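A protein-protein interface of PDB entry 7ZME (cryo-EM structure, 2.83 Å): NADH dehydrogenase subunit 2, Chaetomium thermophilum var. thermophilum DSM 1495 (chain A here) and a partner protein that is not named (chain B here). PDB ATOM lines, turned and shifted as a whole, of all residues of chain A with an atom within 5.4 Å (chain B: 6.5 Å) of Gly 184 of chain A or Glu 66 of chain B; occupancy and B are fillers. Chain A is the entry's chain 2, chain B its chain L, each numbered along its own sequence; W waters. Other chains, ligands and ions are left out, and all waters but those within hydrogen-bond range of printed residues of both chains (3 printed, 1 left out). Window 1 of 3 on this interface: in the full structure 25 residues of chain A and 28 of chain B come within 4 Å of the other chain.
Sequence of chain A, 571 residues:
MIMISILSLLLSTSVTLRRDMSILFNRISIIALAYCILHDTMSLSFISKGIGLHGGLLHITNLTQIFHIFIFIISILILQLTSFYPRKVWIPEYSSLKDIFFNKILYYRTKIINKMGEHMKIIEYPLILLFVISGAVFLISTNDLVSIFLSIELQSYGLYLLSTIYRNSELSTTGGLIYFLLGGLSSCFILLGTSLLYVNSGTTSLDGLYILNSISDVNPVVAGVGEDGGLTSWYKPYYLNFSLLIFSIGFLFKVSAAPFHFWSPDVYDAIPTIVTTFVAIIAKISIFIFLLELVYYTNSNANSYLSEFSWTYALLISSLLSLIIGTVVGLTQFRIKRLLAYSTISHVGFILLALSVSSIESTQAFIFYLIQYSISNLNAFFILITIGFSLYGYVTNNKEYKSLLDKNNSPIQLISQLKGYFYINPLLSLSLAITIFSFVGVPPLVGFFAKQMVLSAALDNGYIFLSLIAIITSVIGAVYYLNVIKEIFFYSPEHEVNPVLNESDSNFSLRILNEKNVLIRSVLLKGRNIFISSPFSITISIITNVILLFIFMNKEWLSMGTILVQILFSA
The backbone carbonyl oxygen (O) of Val 62 of chain B sits at hydrogen-bond distance from the side-chain hydroxyl (OH) of Tyr 157 of chain A (3.4 Å). The side-chain hydroxyl (OH) of Tyr 157 of chain A lies close to the side-chain carboxylate (OE1) of Glu 66 of chain B.
OE2 of Glu 153 of chain A lies within hydrogen-bond range of OH of Tyr 157 of chain A (2.5 Å). O of Gly 184 of chain A is in hydrogen-bond range of SG of Cys 188 of chain A (3.5 Å).
Phe 180 of chain A touches Leu 26 of chain B (CE1 to CD1, 3.7 Å). O of Glu 66 of chain B touches CZ of Phe 180 of chain A (3.2 Å). CZ of Phe 180 of chain A touches CA of Gly 70 of chain B, at 3.4 Å. Phe 15 of chain B touches Leu 181 of chain A (CZ to O, 3.2 Å). CA of Gly 184 of chain A touches OE2 of Glu 66 of chain B (3.6 Å). CB of Leu 185 of chain A touches CE2 of Phe 15 of chain B (3.6 Å). Met 32 of chain B touches Leu 185 of chain A. SG of Cys 188 of chain A touches CB of Met 32 of chain B (3.9 Å). Leu 33 of chain B touches Cys 188 of chain A.
Of the printed residues of chain B, Leu 181 of chain A touches Phe 15. Gly 184 of chain A touches just one residue of chain B: Glu 66. Printed residues of chain B within 4 Å of Leu 185 of chain A: Phe 15 and Met 32. Printed residues of chain A within 4 Å of Leu 26 of chain B: Phe 180. Printed residues of chain A within 4 Å of Leu 33 of chain B: Cys 188 (3.8 Å). Of chain A, only Tyr 157, Phe 180 and Gly 184 come within 4 Å of Glu 66 of chain B. The nearest residue of chain B that does not touch Gly 184 of chain A is Ile 29 of chain B (4.02 Å).
Hydrophobic or aromatic side chains of chain A that line the printed part of chain B: Tyr 157, Phe 180, Leu 181 and Leu 185. Among the printed residues, no Asp or Glu carboxylate lies within 4 Å of a Lys or Arg side-chain nitrogen of the other chain.
Water W1 lies within hydrogen-bond range of the side-chain carboxylate of Glu 66 of chain B (2.8 Å) and the backbone carbonyl oxygen of Phe 180 of chain A (3.4 Å). Water W3 lies within hydrogen-bond range of OE2 of Glu 153 of chain A, OG of Ser 187 of chain A, OE1 of Glu 66 of chain B and OH of Tyr 157 of chain A. Water W2 lies within hydrogen-bond range of O of Gly 184 of chain A (3.1 Å), OE1 of Glu 66 of chain B (3.1 Å) and SG of Cys 188 of chain A (3.7 Å).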
ATOM      1  N   GLU A 153      13.130  -4.408 -20.395  1.00  0.00           N
ATOM      2  CA  GLU A 153      12.846  -5.175 -19.185  1.00  0.00           C
ATOM      3  C   GLU A 153      13.533  -4.569 -17.970  1.00  0.00           C
ATOM      4  O   GLU A 153      12.949  -4.525 -16.883  1.00  0.00           O
ATOM      5  CB  GLU A 153      13.267  -6.631 -19.362  1.00  0.00           C
ATOM      6  CG  GLU A 153      12.516  -7.383 -20.444  1.00  0.00           C
ATOM      7  CD  GLU A 153      11.104  -7.729 -20.038  1.00  0.00           C
ATOM      8  OE1 GLU A 153      10.239  -6.830 -20.061  1.00  0.00           O
ATOM      9  OE2 GLU A 153      10.857  -8.901 -19.692  1.00  0.00           O
ATOM     10  N   TYR A 157      11.100  -3.692 -15.010  1.00  0.00           N
ATOM     11  CA  TYR A 157      11.176  -4.411 -13.742  1.00  0.00           C
ATOM     12  C   TYR A 157      11.420  -3.460 -12.577  1.00  0.00           C
ATOM     13  O   TYR A 157      10.820  -3.610 -11.508  1.00  0.00           O
ATOM     14  CB  TYR A 157      12.277  -5.464 -13.810  1.00  0.00           C
ATOM     15  CG  TYR A 157      11.983  -6.604 -14.753  1.00  0.00           C
ATOM     16  CD1 TYR A 157      10.704  -6.820 -15.238  1.00  0.00           C
ATOM     17  CD2 TYR A 157      12.997  -7.449 -15.179  1.00  0.00           C
ATOM     18  CE1 TYR A 157      10.441  -7.853 -16.105  1.00  0.00           C
ATOM     19  CE2 TYR A 157      12.741  -8.484 -16.050  1.00  0.00           C
ATOM     20  CZ  TYR A 157      11.463  -8.680 -16.505  1.00  0.00           C
ATOM     21  OH  TYR A 157      11.209  -9.711 -17.376  1.00  0.00           O
ATOM     22  N   TYR A 160       8.255  -1.795 -11.673  1.00  0.00           N
ATOM     23  CA  TYR A 160       7.404  -2.668 -10.873  1.00  0.00           C
ATOM     24  C   TYR A 160       7.858  -2.692  -9.423  1.00  0.00           C
ATOM     25  O   TYR A 160       7.030  -2.685  -8.506  1.00  0.00           O
ATOM     26  CB  TYR A 160       7.413  -4.089 -11.438  1.00  0.00           C
ATOM     27  CG  TYR A 160       7.030  -4.200 -12.887  1.00  0.00           C
ATOM     28  CD1 TYR A 160       6.170  -3.287 -13.476  1.00  0.00           C
ATOM     29  CD2 TYR A 160       7.551  -5.212 -13.676  1.00  0.00           C
ATOM     30  CE1 TYR A 160       5.833  -3.392 -14.805  1.00  0.00           C
ATOM     31  CE2 TYR A 160       7.217  -5.325 -14.999  1.00  0.00           C
ATOM     32  CZ  TYR A 160       6.363  -4.414 -15.556  1.00  0.00           C
ATOM     33  OH  TYR A 160       6.043  -4.529 -16.880  1.00  0.00           O
ATOM     34  N   TYR A 179       0.429  -3.400 -12.332  1.00  0.00           N
ATOM     35  CA  TYR A 179       1.418  -2.911 -13.284  1.00  0.00           C
ATOM     36  C   TYR A 179       2.330  -4.038 -13.759  1.00  0.00           C
ATOM     37  O   TYR A 179       2.642  -4.136 -14.950  1.00  0.00           O
ATOM     38  CB  TYR A 179       2.212  -1.772 -12.636  1.00  0.00           C
ATOM     39  CG  TYR A 179       3.078  -0.951 -13.562  1.00  0.00           C
ATOM     40  CD1 TYR A 179       2.912  -0.998 -14.938  1.00  0.00           C
ATOM     41  CD2 TYR A 179       4.020  -0.073 -13.050  1.00  0.00           C
ATOM     42  CE1 TYR A 179       3.692  -0.239 -15.773  1.00  0.00           C
ATOM     43  CE2 TYR A 179       4.799   0.699 -13.878  1.00  0.00           C
ATOM     44  CZ  TYR A 179       4.629   0.614 -15.240  1.00  0.00           C
ATOM     45  OH  TYR A 179       5.406   1.383 -16.073  1.00  0.00           O
ATOM     46  N   PHE A 180       2.755  -4.912 -12.843  1.00  0.00           N
ATOM     47  CA  PHE A 180       3.643  -6.007 -13.222  1.00  0.00           C
ATOM     48  C   PHE A 180       2.944  -6.986 -14.158  1.00  0.00           C
ATOM     49  O   PHE A 180       3.516  -7.412 -15.167  1.00  0.00           O
ATOM     50  CB  PHE A 180       4.158  -6.738 -11.979  1.00  0.00           C
ATOM     51  CG  PHE A 180       4.845  -8.042 -12.287  1.00  0.00           C
ATOM     52  CD1 PHE A 180       4.125  -9.224 -12.379  1.00  0.00           C
ATOM     53  CD2 PHE A 180       6.206  -8.080 -12.508  1.00  0.00           C
ATOM     54  CE1 PHE A 180       4.749 -10.404 -12.684  1.00  0.00           C
ATOM     55  CE2 PHE A 180       6.834  -9.259 -12.812  1.00  0.00           C
ATOM     56  CZ  PHE A 180       6.105 -10.423 -12.903  1.00  0.00           C
ATOM     57  N   LEU A 181       1.710  -7.372 -13.825  1.00  0.00           N
ATOM     58  CA  LEU A 181       1.002  -8.367 -14.625  1.00  0.00           C
ATOM     59  C   LEU A 181       0.693  -7.841 -16.017  1.00  0.00           C
ATOM     60  O   LEU A 181       0.944  -8.518 -17.019  1.00  0.00           O
ATOM     61  CB  LEU A 181      -0.287  -8.788 -13.927  1.00  0.00           C
ATOM     62  CG  LEU A 181      -0.236  -9.924 -12.908  1.00  0.00           C
ATOM     63  CD1 LEU A 181      -1.613 -10.124 -12.332  1.00  0.00           C
ATOM     64  CD2 LEU A 181       0.276 -11.210 -13.525  1.00  0.00           C
ATOM     65  N   LEU A 182       0.138  -6.633 -16.100  1.00  0.00           N
ATOM     66  CA  LEU A 182      -0.238  -6.085 -17.395  1.00  0.00           C
ATOM     67  C   LEU A 182       0.981  -5.648 -18.191  1.00  0.00           C
ATOM     68  O   LEU A 182       0.952  -5.662 -19.425  1.00  0.00           O
ATOM     69  CB  LEU A 182      -1.196  -4.915 -17.209  1.00  0.00           C
ATOM     70  CG  LEU A 182      -2.647  -5.220 -16.855  1.00  0.00           C
ATOM     71  CD1 LEU A 182      -3.470  -3.979 -17.077  1.00  0.00           C
ATOM     72  CD2 LEU A 182      -3.185  -6.380 -17.669  1.00  0.00           C
ATOM     73  N   GLY A 183       2.054  -5.246 -17.507  1.00  0.00           N
ATOM     74  CA  GLY A 183       3.299  -4.975 -18.194  1.00  0.00           C
ATOM     75  C   GLY A 183       4.032  -6.211 -18.658  1.00  0.00           C
ATOM     76  O   GLY A 183       4.799  -6.136 -19.621  1.00  0.00           O
ATOM     77  N   GLY A 184       3.826  -7.344 -17.984  1.00  0.00           N
ATOM     78  CA  GLY A 184       4.362  -8.597 -18.484  1.00  0.00           C
ATOM     79  C   GLY A 184       3.681  -9.032 -19.765  1.00  0.00           C
ATOM     80  O   GLY A 184       4.319  -9.587 -20.663  1.00  0.00           O
ATOM     81  N   LEU A 185       2.372  -8.803 -19.857  1.00  0.00           N
ATOM     82  CA  LEU A 185       1.667  -9.002 -21.116  1.00  0.00           C
ATOM     83  C   LEU A 185       2.181  -8.047 -22.183  1.00  0.00           C
ATOM     84  O   LEU A 185       2.233  -8.393 -23.367  1.00  0.00           O
ATOM     85  CB  LEU A 185       0.168  -8.813 -20.902  1.00  0.00           C
ATOM     86  CG  LEU A 185      -0.723  -9.032 -22.123  1.00  0.00           C
ATOM     87  CD1 LEU A 185      -0.762 -10.503 -22.456  1.00  0.00           C
ATOM     88  CD2 LEU A 185      -2.121  -8.493 -21.878  1.00  0.00           C
ATOM     89  N   SER A 186       2.549  -6.829 -21.778  1.00  0.00           N
ATOM     90  CA  SER A 186       3.098  -5.856 -22.713  1.00  0.00           C
ATOM     91  C   SER A 186       4.424  -6.331 -23.291  1.00  0.00           C
ATOM     92  O   SER A 186       4.705  -6.121 -24.476  1.00  0.00           O
ATOM     93  CB  SER A 186       3.268  -4.509 -22.009  1.00  0.00           C
ATOM     94  OG  SER A 186       3.829  -3.535 -22.867  1.00  0.00           O
ATOM     95  N   SER A 187       5.254  -6.968 -22.468  1.00  0.00           N
ATOM     96  CA  SER A 187       6.552  -7.433 -22.942  1.00  0.00           C
ATOM     97  C   SER A 187       6.420  -8.649 -23.849  1.00  0.00           C
ATOM     98  O   SER A 187       7.282  -8.878 -24.703  1.00  0.00           O
ATOM     99  CB  SER A 187       7.455  -7.747 -21.752  1.00  0.00           C
ATOM    100  OG  SER A 187       7.518  -6.646 -20.867  1.00  0.00           O
ATOM    101  N   CYS A 188       5.360  -9.439 -23.681  1.00  0.00           N
ATOM    102  CA  CYS A 188       5.159 -10.595 -24.545  1.00  0.00           C
ATOM    103  C   CYS A 188       4.836 -10.166 -25.969  1.00  0.00           C
ATOM    104  O   CYS A 188       5.085 -10.914 -26.920  1.00  0.00           O
ATOM    105  CB  CYS A 188       4.052 -11.488 -23.985  1.00  0.00           C
ATOM    106  SG  CYS A 188       4.552 -12.520 -22.598  1.00  0.00           S
ATOM    107  N   PHE B  15      -3.834 -16.235 -19.562  1.00  0.00           N
ATOM    108  CA  PHE B  15      -3.586 -14.978 -18.869  1.00  0.00           C
ATOM    109  C   PHE B  15      -4.813 -14.080 -18.873  1.00  0.00           C
ATOM    110  O   PHE B  15      -5.143 -13.468 -17.854  1.00  0.00           O
ATOM    111  CB  PHE B  15      -2.401 -14.252 -19.519  1.00  0.00           C
ATOM    112  CG  PHE B  15      -2.078 -12.930 -18.890  1.00  0.00           C
ATOM    113  CD1 PHE B  15      -1.287 -12.863 -17.754  1.00  0.00           C
ATOM    114  CD2 PHE B  15      -2.563 -11.751 -19.434  1.00  0.00           C
ATOM    115  CE1 PHE B  15      -0.983 -11.650 -17.169  1.00  0.00           C
ATOM    116  CE2 PHE B  15      -2.269 -10.533 -18.853  1.00  0.00           C
ATOM    117  CZ  PHE B  15      -1.475 -10.482 -17.720  1.00  0.00           C
ATOM    118  N   LEU B  26       0.824 -15.677 -13.815  1.00  0.00           N
ATOM    119  CA  LEU B  26       2.307 -15.654 -13.935  1.00  0.00           C
ATOM    120  C   LEU B  26       2.803 -16.897 -14.694  1.00  0.00           C
ATOM    121  O   LEU B  26       3.848 -16.791 -15.349  1.00  0.00           O
ATOM    122  CB  LEU B  26       2.859 -15.603 -12.507  1.00  0.00           C
ATOM    123  CG  LEU B  26       4.363 -15.399 -12.352  1.00  0.00           C
ATOM    124  CD1 LEU B  26       4.808 -14.094 -12.991  1.00  0.00           C
ATOM    125  CD2 LEU B  26       4.747 -15.424 -10.883  1.00  0.00           C
ATOM    126  N   ILE B  29       2.202 -16.208 -18.566  1.00  0.00           N
ATOM    127  CA  ILE B  29       3.312 -15.442 -19.122  1.00  0.00           C
ATOM    128  C   ILE B  29       4.478 -16.368 -19.441  1.00  0.00           C
ATOM    129  O   ILE B  29       5.130 -16.236 -20.483  1.00  0.00           O
ATOM    130  CB  ILE B  29       3.723 -14.322 -18.149  1.00  0.00           C
ATOM    131  CG1 ILE B  29       2.672 -13.212 -18.138  1.00  0.00           C
ATOM    132  CG2 ILE B  29       5.082 -13.759 -18.518  1.00  0.00           C
ATOM    133  CD1 ILE B  29       2.952 -12.114 -17.134  1.00  0.00           C
ATOM    134  N   MET B  32       3.835 -18.240 -22.707  1.00  0.00           N
ATOM    135  CA  MET B  32       4.030 -17.398 -23.883  1.00  0.00           C
ATOM    136  C   MET B  32       5.507 -17.229 -24.206  1.00  0.00           C
ATOM    137  O   MET B  32       5.908 -17.315 -25.372  1.00  0.00           O
ATOM    138  CB  MET B  32       3.379 -16.036 -23.665  1.00  0.00           C
ATOM    139  CG  MET B  32       1.882 -16.090 -23.548  1.00  0.00           C
ATOM    140  SD  MET B  32       1.109 -14.490 -23.774  1.00  0.00           S
ATOM    141  CE  MET B  32       0.763 -14.056 -22.077  1.00  0.00           C
ATOM    142  N   LEU B  33       6.329 -16.985 -23.186  1.00  0.00           N
ATOM    143  CA  LEU B  33       7.763 -16.869 -23.403  1.00  0.00           C
ATOM    144  C   LEU B  33       8.352 -18.180 -23.903  1.00  0.00           C
ATOM    145  O   LEU B  33       9.273 -18.167 -24.726  1.00  0.00           O
ATOM    146  CB  LEU B  33       8.448 -16.419 -22.116  1.00  0.00           C
ATOM    147  CG  LEU B  33       8.042 -15.020 -21.643  1.00  0.00           C
ATOM    148  CD1 LEU B  33       8.926 -14.542 -20.516  1.00  0.00           C
ATOM    149  CD2 LEU B  33       8.053 -14.029 -22.786  1.00  0.00           C
ATOM    150  N   VAL B  61      16.729 -16.286 -19.132  1.00  0.00           N
ATOM    151  CA  VAL B  61      17.251 -15.667 -17.917  1.00  0.00           C
ATOM    152  C   VAL B  61      16.355 -14.519 -17.465  1.00  0.00           C
ATOM    153  O   VAL B  61      16.155 -14.313 -16.263  1.00  0.00           O
ATOM    154  CB  VAL B  61      18.718 -15.223 -18.105  1.00  0.00           C
ATOM    155  CG1 VAL B  61      18.838 -14.041 -19.043  1.00  0.00           C
ATOM    156  CG2 VAL B  61      19.339 -14.900 -16.773  1.00  0.00           C
ATOM    157  N   VAL B  62      15.798 -13.756 -18.408  1.00  0.00           N
ATOM    158  CA  VAL B  62      14.870 -12.694 -18.027  1.00  0.00           C
ATOM    159  C   VAL B  62      13.505 -13.273 -17.679  1.00  0.00           C
ATOM    160  O   VAL B  62      12.757 -12.696 -16.884  1.00  0.00           O
ATOM    161  CB  VAL B  62      14.771 -11.625 -19.131  1.00  0.00           C
ATOM    162  CG1 VAL B  62      16.155 -11.144 -19.535  1.00  0.00           C
ATOM    163  CG2 VAL B  62      14.021 -12.161 -20.327  1.00  0.00           C
ATOM    164  N   ALA B  63      13.158 -14.417 -18.267  1.00  0.00           N
ATOM    165  CA  ALA B  63      11.904 -15.068 -17.912  1.00  0.00           C
ATOM    166  C   ALA B  63      11.919 -15.526 -16.462  1.00  0.00           C
ATOM    167  O   ALA B  63      10.888 -15.481 -15.780  1.00  0.00           O
ATOM    168  CB  ALA B  63      11.642 -16.249 -18.845  1.00  0.00           C
ATOM    169  N   GLY B  64      13.076 -15.979 -15.976  1.00  0.00           N
ATOM    170  CA  GLY B  64      13.181 -16.355 -14.578  1.00  0.00           C
ATOM    171  C   GLY B  64      13.288 -15.155 -13.662  1.00  0.00           C
ATOM    172  O   GLY B  64      12.785 -15.178 -12.537  1.00  0.00           O
ATOM    173  N   ALA B  65      13.946 -14.093 -14.129  1.00  0.00           N
ATOM    174  CA  ALA B  65      14.003 -12.858 -13.355  1.00  0.00           C
ATOM    175  C   ALA B  65      12.616 -12.251 -13.197  1.00  0.00           C
ATOM    176  O   ALA B  65      12.279 -11.717 -12.135  1.00  0.00           O
ATOM    177  CB  ALA B  65      14.956 -11.866 -14.017  1.00  0.00           C
ATOM    178  N   GLU B  66      11.799 -12.318 -14.248  1.00  0.00           N
ATOM    179  CA  GLU B  66      10.431 -11.823 -14.160  1.00  0.00           C
ATOM    180  C   GLU B  66       9.597 -12.668 -13.205  1.00  0.00           C
ATOM    181  O   GLU B  66       8.747 -12.139 -12.481  1.00  0.00           O
ATOM    182  CB  GLU B  66       9.799 -11.792 -15.552  1.00  0.00           C
ATOM    183  CG  GLU B  66       8.295 -11.607 -15.555  1.00  0.00           C
ATOM    184  CD  GLU B  66       7.727 -11.496 -16.952  1.00  0.00           C
ATOM    185  OE1 GLU B  66       8.478 -11.742 -17.918  1.00  0.00           O
ATOM    186  OE2 GLU B  66       6.533 -11.159 -17.085  1.00  0.00           O
ATOM    187  N   SER B  67       9.829 -13.980 -13.184  1.00  0.00           N
ATOM    188  CA  SER B  67       9.063 -14.845 -12.295  1.00  0.00           C
ATOM    189  C   SER B  67       9.480 -14.674 -10.841  1.00  0.00           C
ATOM    190  O   SER B  67       8.685 -14.945  -9.936  1.00  0.00           O
ATOM    191  CB  SER B  67       9.202 -16.304 -12.734  1.00  0.00           C
ATOM    192  OG  SER B  67      10.524 -16.772 -12.553  1.00  0.00           O
ATOM    193  N   ALA B  68      10.712 -14.228 -10.593  1.00  0.00           N
ATOM    194  CA  ALA B  68      11.128 -13.915  -9.232  1.00  0.00           C
ATOM    195  C   ALA B  68      10.504 -12.615  -8.741  1.00  0.00           C
ATOM    196  O   ALA B  68      10.061 -12.532  -7.591  1.00  0.00           O
ATOM    197  CB  ALA B  68      12.651 -13.839  -9.150  1.00  0.00           C
ATOM    198  N   ILE B  69      10.468 -11.589  -9.592  1.00  0.00           N
ATOM    199  CA  ILE B  69       9.824 -10.334  -9.221  1.00  0.00           C
ATOM    200  C   ILE B  69       8.322 -10.529  -9.076  1.00  0.00           C
ATOM    201  O   ILE B  69       7.687  -9.930  -8.202  1.00  0.00           O
ATOM    202  CB  ILE B  69      10.165  -9.237 -10.247  1.00  0.00           C
ATOM    203  CG1 ILE B  69      11.676  -9.074 -10.356  1.00  0.00           C
ATOM    204  CG2 ILE B  69       9.522  -7.914  -9.868  1.00  0.00           C
ATOM    205  CD1 ILE B  69      12.316  -8.621  -9.078  1.00  0.00           C
ATOM    206  N   GLY B  70       7.731 -11.372  -9.922  1.00  0.00           N
ATOM    207  CA  GLY B  70       6.314 -11.659  -9.791  1.00  0.00           C
ATOM    208  C   GLY B  70       5.976 -12.406  -8.517  1.00  0.00           C
ATOM    209  O   GLY B  70       4.997 -12.083  -7.841  1.00  0.00           O
ATOM    210  N   LEU B  71       6.771 -13.420  -8.176  1.00  0.00           N
ATOM    211  CA  LEU B  71       6.522 -14.157  -6.944  1.00  0.00           C
ATOM    212  C   LEU B  71       6.797 -13.289  -5.725  1.00  0.00           C
ATOM    213  O   LEU B  71       6.107 -13.401  -4.708  1.00  0.00           O
ATOM    214  CB  LEU B  71       7.369 -15.429  -6.909  1.00  0.00           C
ATOM    215  CG  LEU B  71       6.822 -16.606  -7.721  1.00  0.00           C
ATOM    216  CD1 LEU B  71       7.694 -17.826  -7.557  1.00  0.00           C
ATOM    217  CD2 LEU B  71       5.389 -16.914  -7.329  1.00  0.00           C
HETATM  218  O   HOH W   1       6.627  -8.606 -15.970  1.00  0.00           O
HETATM  219  O   HOH W   2       7.167 -10.808 -20.603  1.00  0.00           O
HETATM  220  O   HOH W   3       8.170  -8.508 -18.403  1.00  0.00           O
